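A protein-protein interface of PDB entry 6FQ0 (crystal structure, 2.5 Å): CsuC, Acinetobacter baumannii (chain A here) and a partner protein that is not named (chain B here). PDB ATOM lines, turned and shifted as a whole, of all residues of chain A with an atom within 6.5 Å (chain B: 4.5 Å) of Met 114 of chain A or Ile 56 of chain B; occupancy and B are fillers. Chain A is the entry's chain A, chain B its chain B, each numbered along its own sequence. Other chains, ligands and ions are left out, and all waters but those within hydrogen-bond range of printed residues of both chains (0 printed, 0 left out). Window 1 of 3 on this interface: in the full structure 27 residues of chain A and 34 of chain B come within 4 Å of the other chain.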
ATOM      1  N   ALA A   1     -30.660  -6.671  -5.227  1.00  0.00           N
ATOM      2  CA  ALA A   1     -31.072  -6.425  -6.603  1.00  0.00           C
ATOM      3  C   ALA A   1     -31.734  -7.662  -7.203  1.00  0.00           C
ATOM      4  O   ALA A   1     -31.640  -8.761  -6.650  1.00  0.00           O
ATOM      5  CB  ALA A   1     -29.880  -5.997  -7.446  1.00  0.00           C
ATOM      6  N   VAL A  92     -21.961 -16.072  -9.730  1.00  0.00           N
ATOM      7  CA  VAL A  92     -22.248 -14.649  -9.857  1.00  0.00           C
ATOM      8  C   VAL A  92     -22.340 -14.077  -8.450  1.00  0.00           C
ATOM      9  O   VAL A  92     -23.280 -14.388  -7.705  1.00  0.00           O
ATOM     10  CB  VAL A  92     -23.536 -14.392 -10.648  1.00  0.00           C
ATOM     11  CG1 VAL A  92     -23.735 -12.902 -10.856  1.00  0.00           C
ATOM     12  CG2 VAL A  92     -23.491 -15.118 -11.982  1.00  0.00           C
ATOM     13  N   ASP A  93     -21.370 -13.247  -8.079  1.00  0.00           N
ATOM     14  CA  ASP A  93     -21.332 -12.618  -6.766  1.00  0.00           C
ATOM     15  C   ASP A  93     -21.809 -11.177  -6.887  1.00  0.00           C
ATOM     16  O   ASP A  93     -21.163 -10.361  -7.552  1.00  0.00           O
ATOM     17  CB  ASP A  93     -19.921 -12.664  -6.179  1.00  0.00           C
ATOM     18  CG  ASP A  93     -19.557 -14.029  -5.637  1.00  0.00           C
ATOM     19  OD1 ASP A  93     -20.416 -14.658  -4.985  1.00  0.00           O
ATOM     20  OD2 ASP A  93     -18.410 -14.473  -5.854  1.00  0.00           O
ATOM     21  N   GLU A  94     -22.924 -10.862  -6.232  1.00  0.00           N
ATOM     22  CA  GLU A  94     -23.452  -9.504  -6.240  1.00  0.00           C
ATOM     23  C   GLU A  94     -22.707  -8.672  -5.203  1.00  0.00           C
ATOM     24  O   GLU A  94     -22.784  -8.950  -4.002  1.00  0.00           O
ATOM     25  CB  GLU A  94     -24.952  -9.505  -5.957  1.00  0.00           C
ATOM     26  CG  GLU A  94     -25.613  -8.147  -6.141  1.00  0.00           C
ATOM     27  CD  GLU A  94     -26.728  -7.895  -5.143  1.00  0.00           C
ATOM     28  OE1 GLU A  94     -26.885  -8.705  -4.204  1.00  0.00           O
ATOM     29  OE2 GLU A  94     -27.445  -6.884  -5.295  1.00  0.00           O
ATOM     30  N   LEU A  95     -21.983  -7.660  -5.669  1.00  0.00           N
ATOM     31  CA  LEU A  95     -21.177  -6.818  -4.795  1.00  0.00           C
ATOM     32  C   LEU A  95     -21.979  -5.603  -4.333  1.00  0.00           C
ATOM     33  O   LEU A  95     -22.670  -4.973  -5.138  1.00  0.00           O
ATOM     34  CB  LEU A  95     -19.912  -6.355  -5.512  1.00  0.00           C
ATOM     35  CG  LEU A  95     -19.223  -7.415  -6.374  1.00  0.00           C
ATOM     36  CD1 LEU A  95     -18.029  -6.827  -7.113  1.00  0.00           C
ATOM     37  CD2 LEU A  95     -18.801  -8.613  -5.532  1.00  0.00           C
ATOM     38  N   PHE A 112     -27.383  -8.549   3.542  1.00  0.00           N
ATOM     39  CA  PHE A 112     -27.236  -9.759   2.747  1.00  0.00           C
ATOM     40  C   PHE A 112     -26.355  -9.493   1.535  1.00  0.00           C
ATOM     41  O   PHE A 112     -26.448  -8.434   0.906  1.00  0.00           O
ATOM     42  CB  PHE A 112     -28.596 -10.281   2.281  1.00  0.00           C
ATOM     43  CG  PHE A 112     -29.530 -10.624   3.402  1.00  0.00           C
ATOM     44  CD1 PHE A 112     -29.043 -11.083   4.613  1.00  0.00           C
ATOM     45  CD2 PHE A 112     -30.898 -10.484   3.245  1.00  0.00           C
ATOM     46  CE1 PHE A 112     -29.902 -11.397   5.646  1.00  0.00           C
ATOM     47  CE2 PHE A 112     -31.762 -10.796   4.274  1.00  0.00           C
ATOM     48  CZ  PHE A 112     -31.263 -11.251   5.477  1.00  0.00           C
ATOM     49  N   GLN A 113     -25.500 -10.460   1.213  1.00  0.00           N
ATOM     50  CA  GLN A 113     -24.725 -10.458  -0.022  1.00  0.00           C
ATOM     51  C   GLN A 113     -25.125 -11.687  -0.823  1.00  0.00           C
ATOM     52  O   GLN A 113     -24.970 -12.817  -0.350  1.00  0.00           O
ATOM     53  CB  GLN A 113     -23.222 -10.453   0.262  1.00  0.00           C
ATOM     54  CG  GLN A 113     -22.383  -9.940  -0.898  1.00  0.00           C
ATOM     55  CD  GLN A 113     -20.896 -10.102  -0.659  1.00  0.00           C
ATOM     56  OE1 GLN A 113     -20.436 -11.161  -0.235  1.00  0.00           O
ATOM     57  NE2 GLN A 113     -20.135  -9.047  -0.927  1.00  0.00           N
ATOM     58  N   MET A 114     -25.635 -11.465  -2.031  1.00  0.00           N
ATOM     59  CA  MET A 114     -26.177 -12.544  -2.844  1.00  0.00           C
ATOM     60  C   MET A 114     -25.086 -13.178  -3.697  1.00  0.00           C
ATOM     61  O   MET A 114     -24.278 -12.475  -4.312  1.00  0.00           O
ATOM     62  CB  MET A 114     -27.309 -12.024  -3.730  1.00  0.00           C
ATOM     63  CG  MET A 114     -28.457 -11.399  -2.956  1.00  0.00           C
ATOM     64  SD  MET A 114     -29.083 -12.488  -1.662  1.00  0.00           S
ATOM     65  CE  MET A 114     -29.756 -13.826  -2.646  1.00  0.00           C
ATOM     66  N   ARG A 115     -25.062 -14.509  -3.718  1.00  0.00           N
ATOM     67  CA  ARG A 115     -24.241 -15.280  -4.639  1.00  0.00           C
ATOM     68  C   ARG A 115     -25.138 -16.274  -5.356  1.00  0.00           C
ATOM     69  O   ARG A 115     -25.877 -17.025  -4.710  1.00  0.00           O
ATOM     70  CB  ARG A 115     -23.107 -16.015  -3.915  1.00  0.00           C
ATOM     71  CG  ARG A 115     -22.606 -17.242  -4.667  1.00  0.00           C
ATOM     72  CD  ARG A 115     -21.353 -17.824  -4.039  1.00  0.00           C
ATOM     73  NE  ARG A 115     -20.226 -16.899  -4.115  1.00  0.00           N
ATOM     74  CZ  ARG A 115     -18.986 -17.202  -3.747  1.00  0.00           C
ATOM     75  NH1 ARG A 115     -18.710 -18.409  -3.273  1.00  0.00           N
ATOM     76  NH2 ARG A 115     -18.022 -16.299  -3.855  1.00  0.00           N
ATOM     77  N   TYR A 116     -25.079 -16.277  -6.683  1.00  0.00           N
ATOM     78  CA  TYR A 116     -25.892 -17.168  -7.497  1.00  0.00           C
ATOM     79  C   TYR A 116     -24.998 -18.157  -8.233  1.00  0.00           C
ATOM     80  O   TYR A 116     -24.035 -17.757  -8.897  1.00  0.00           O
ATOM     81  CB  TYR A 116     -26.748 -16.368  -8.479  1.00  0.00           C
ATOM     82  CG  TYR A 116     -27.618 -15.343  -7.787  1.00  0.00           C
ATOM     83  CD1 TYR A 116     -28.723 -15.734  -7.042  1.00  0.00           C
ATOM     84  CD2 TYR A 116     -27.329 -13.986  -7.866  1.00  0.00           C
ATOM     85  CE1 TYR A 116     -29.519 -14.805  -6.397  1.00  0.00           C
ATOM     86  CE2 TYR A 116     -28.121 -13.049  -7.225  1.00  0.00           C
ATOM     87  CZ  TYR A 116     -29.214 -13.465  -6.494  1.00  0.00           C
ATOM     88  OH  TYR A 116     -30.005 -12.537  -5.855  1.00  0.00           O
ATOM     89  N   GLY B  16     -33.622 -12.854  -6.490  1.00  0.00           N
ATOM     90  CA  GLY B  16     -33.537 -11.625  -5.730  1.00  0.00           C
ATOM     91  C   GLY B  16     -34.760 -11.504  -4.847  1.00  0.00           C
ATOM     92  O   GLY B  16     -35.421 -12.512  -4.584  1.00  0.00           O
ATOM     93  N   GLY B  17     -35.108 -10.296  -4.419  1.00  0.00           N
ATOM     94  CA  GLY B  17     -34.462  -9.084  -4.879  1.00  0.00           C
ATOM     95  C   GLY B  17     -35.491  -8.010  -5.180  1.00  0.00           C
ATOM     96  O   GLY B  17     -36.635  -8.317  -5.520  1.00  0.00           O
ATOM     97  N   VAL B  47     -36.741 -10.653   6.805  1.00  0.00           N
ATOM     98  CA  VAL B  47     -36.839 -10.331   5.383  1.00  0.00           C
ATOM     99  C   VAL B  47     -37.602 -11.503   4.763  1.00  0.00           C
ATOM    100  O   VAL B  47     -37.005 -12.473   4.286  1.00  0.00           O
ATOM    101  CB  VAL B  47     -35.471 -10.138   4.721  1.00  0.00           C
ATOM    102  CG1 VAL B  47     -35.625  -9.832   3.238  1.00  0.00           C
ATOM    103  CG2 VAL B  47     -34.697  -9.030   5.423  1.00  0.00           C
ATOM    104  N   ASN B  55     -38.534  -9.246   0.267  1.00  0.00           N
ATOM    105  CA  ASN B  55     -37.921 -10.531   0.569  1.00  0.00           C
ATOM    106  C   ASN B  55     -37.175 -11.027  -0.658  1.00  0.00           C
ATOM    107  O   ASN B  55     -37.266 -10.451  -1.746  1.00  0.00           O
ATOM    108  CB  ASN B  55     -38.965 -11.556   1.018  1.00  0.00           C
ATOM    109  CG  ASN B  55     -40.015 -11.820  -0.043  1.00  0.00           C
ATOM    110  OD1 ASN B  55     -41.064 -11.178  -0.067  1.00  0.00           O
ATOM    111  ND2 ASN B  55     -39.746 -12.783  -0.919  1.00  0.00           N
ATOM    112  N   ILE B  56     -36.430 -12.110  -0.461  1.00  0.00           N
ATOM    113  CA  ILE B  56     -35.758 -12.829  -1.535  1.00  0.00           C
ATOM    114  C   ILE B  56     -36.706 -13.891  -2.073  1.00  0.00           C
ATOM    115  O   ILE B  56     -37.386 -14.578  -1.302  1.00  0.00           O
ATOM    116  CB  ILE B  56     -34.444 -13.456  -1.032  1.00  0.00           C
ATOM    117  CG1 ILE B  56     -33.582 -12.394  -0.346  1.00  0.00           C
ATOM    118  CG2 ILE B  56     -33.682 -14.099  -2.178  1.00  0.00           C
ATOM    119  CD1 ILE B  56     -32.394 -12.960   0.399  1.00  0.00           C
ATOM    120  N   SER B  57     -36.747 -14.043  -3.397  1.00  0.00           N
ATOM    121  CA  SER B  57     -37.625 -15.029  -4.011  1.00  0.00           C
ATOM    122  C   SER B  57     -37.010 -15.532  -5.309  1.00  0.00           C
ATOM    123  O   SER B  57     -36.093 -14.921  -5.863  1.00  0.00           O
ATOM    124  CB  SER B  57     -39.020 -14.451  -4.275  1.00  0.00           C
ATOM    125  OG  SER B  57     -39.024 -13.635  -5.433  1.00  0.00           O
ATOM    126  N   THR B 121     -41.296 -18.454  -5.365  1.00  0.00           N
ATOM    127  CA  THR B 121     -40.942 -19.160  -4.139  1.00  0.00           C
ATOM    128  C   THR B 121     -40.108 -18.217  -3.281  1.00  0.00           C
ATOM    129  O   THR B 121     -38.987 -17.856  -3.654  1.00  0.00           O
ATOM    130  CB  THR B 121     -40.174 -20.446  -4.441  1.00  0.00           C
ATOM    131  OG1 THR B 121     -41.020 -21.354  -5.160  1.00  0.00           O
ATOM    132  CG2 THR B 121     -39.710 -21.105  -3.148  1.00  0.00           C
ATOM    133  N   ALA B 122     -40.653 -17.823  -2.134  1.00  0.00           N
ATOM    134  CA  ALA B 122     -39.926 -16.941  -1.235  1.00  0.00           C
ATOM    135  C   ALA B 122     -38.785 -17.687  -0.557  1.00  0.00           C
ATOM    136  O   ALA B 122     -38.861 -18.891  -0.301  1.00  0.00           O
ATOM    137  CB  ALA B 122     -40.864 -16.354  -0.181  1.00  0.00           C
ATOM    138  N   VAL B 123     -37.715 -16.954  -0.273  1.00  0.00           N
ATOM    139  CA  VAL B 123     -36.626 -17.463   0.552  1.00  0.00           C
ATOM    140  C   VAL B 123     -36.690 -16.687   1.862  1.00  0.00           C
ATOM    141  O   VAL B 123     -35.977 -15.687   2.030  1.00  0.00           O
ATOM    142  CB  VAL B 123     -35.266 -17.315  -0.148  1.00  0.00           C
ATOM    143  CG1 VAL B 123     -34.144 -17.852   0.737  1.00  0.00           C
ATOM    144  CG2 VAL B 123     -35.285 -18.019  -1.502  1.00  0.00           C
ATOM    145  N   ILE B 125     -36.316 -15.212   5.588  1.00  0.00           N
ATOM    146  CA  ILE B 125     -35.168 -15.063   6.471  1.00  0.00           C
ATOM    147  C   ILE B 125     -35.646 -14.356   7.731  1.00  0.00           C
ATOM    148  O   ILE B 125     -36.011 -13.175   7.686  1.00  0.00           O
ATOM    149  CB  ILE B 125     -34.024 -14.288   5.805  1.00  0.00           C
ATOM    150  CG1 ILE B 125     -33.403 -15.118   4.677  1.00  0.00           C
ATOM    151  CG2 ILE B 125     -32.984 -13.884   6.831  1.00  0.00           C
ATOM    152  CD1 ILE B 125     -32.317 -14.397   3.911  1.00  0.00           C
ATOM    153  N   VAL B 148     -25.549 -15.121   1.196  1.00  0.00           N
ATOM    154  CA  VAL B 148     -26.683 -15.981   0.884  1.00  0.00           C
ATOM    155  C   VAL B 148     -26.434 -16.572  -0.496  1.00  0.00           C
ATOM    156  O   VAL B 148     -26.471 -15.858  -1.505  1.00  0.00           O
ATOM    157  CB  VAL B 148     -28.012 -15.215   0.933  1.00  0.00           C
ATOM    158  CG1 VAL B 148     -29.165 -16.126   0.524  1.00  0.00           C
ATOM    159  CG2 VAL B 148     -28.236 -14.639   2.326  1.00  0.00           C
ATOM    160  N   VAL B 150     -27.500 -19.029  -3.475  1.00  0.00           N
ATOM    161  CA  VAL B 150     -28.585 -19.749  -4.129  1.00  0.00           C
ATOM    162  C   VAL B 150     -27.971 -20.650  -5.191  1.00  0.00           C
ATOM    163  O   VAL B 150     -27.323 -20.170  -6.128  1.00  0.00           O
ATOM    164  CB  VAL B 150     -29.611 -18.784  -4.741  1.00  0.00           C
ATOM    165  CG1 VAL B 150     -30.797 -19.554  -5.304  1.00  0.00           C
ATOM    166  CG2 VAL B 150     -30.068 -17.770  -3.700  1.00  0.00           C
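Hydrophobic or aromatic side chains of chain B within 4 Å of the printed part of chain A: Val 47, Ile 56, Ile 125, Val 148 and Val 150. Of the 10 printed residues of chain A, 6 touch a printed residue of chain B. Printed residues of chain A that touch a printed residue of chain B: Ala 1, Phe 112, Gln 113, Met 114, Arg 115 and Tyr 116. Among the printed residues, 11 pairs touch across the chains. Among the printed residues, no Asp or Glu carboxylate lies within 4 Å of a Lys or Arg side-chain nitrogen of the other chain.
The backbone carbonyl oxygen (O) of Val 148 of chain B sits at hydrogen-bond distance from the backbone NH (N) of Arg 115 of chain A. O of Gln 113 of chain A lies within hydrogen-bond range of N of Val 148 of chain B, 2.8 Å away. N of Val 150 of chain B lies within hydrogen-bond range of O of Arg 115 of chain A.
The backbone NH (N) of Gly 16 of chain B sits at hydrogen-bond distance from the backbone carbonyl oxygen (O) of Ser 57 of chain B, 3.3 Å away. N of Val 123 of chain B sits at hydrogen-bond distance from O of Ile 56 of chain B (2.6 Å). OD1 of Asp 93 of chain A lies within salt-bridge range of NE of Arg 115 of chain A (2.4 Å). The backbone NH of Glu 94 of chain A is in hydrogen-bond range of the backbone carbonyl oxygen of Met 114 of chain A (2.8 Å). O of Asn 55 of chain B lies within hydrogen-bond range of N of Gly 17 of chain B (3.4 Å). N of Val 47 of chain B sits at hydrogen-bond distance from O of Ile 125 of chain B (2.8 Å).
Of chain B, only Ile 56 (3.9 Å) and Val 148 (3.6 Å) come within 4 Å of Met 114 of chain A. Ile 56 of chain B touches one residue of chain A. Printed residues of chain A within 4 Å of Val 148 of chain B: Gln 113 (2.8 Å), Met 114 (3.6 Å) and Arg 115 (2.9 Å). Printed residues of chain B within 4 Å of Tyr 116 of chain A: Gly 16 and Val 150. The nearest residue of chain A that does not touch Ile 56 of chain B is Phe 112 of chain A (4.1 Å). The nearest printed residue of chain B that does not touch Phe 112 of chain A is Ile 56 of chain B (4.1 Å).
Ala 1 of chain A touches Gly 16 of chain B. Gly 17 of chain B touches Ala 1 of chain A (CA to O, 3.3 Å). CE2 of Phe 112 of chain A touches CG2 of Val 47 of chain B, 3.6 Å away. CG2 of Ile 125 of chain B touches CZ of Phe 112 of chain A, at 3.4 Å. Ile 56 of chain B touches Met 114 of chain A. CA of Met 114 of chain A touches O of Val 148 of chain B, at 3.6 Å. Gly 16 of chain B touches Tyr 116 of chain A. O of Val 150 of chain B touches CA of Tyr 116 of chain A, at 3.6 Å.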
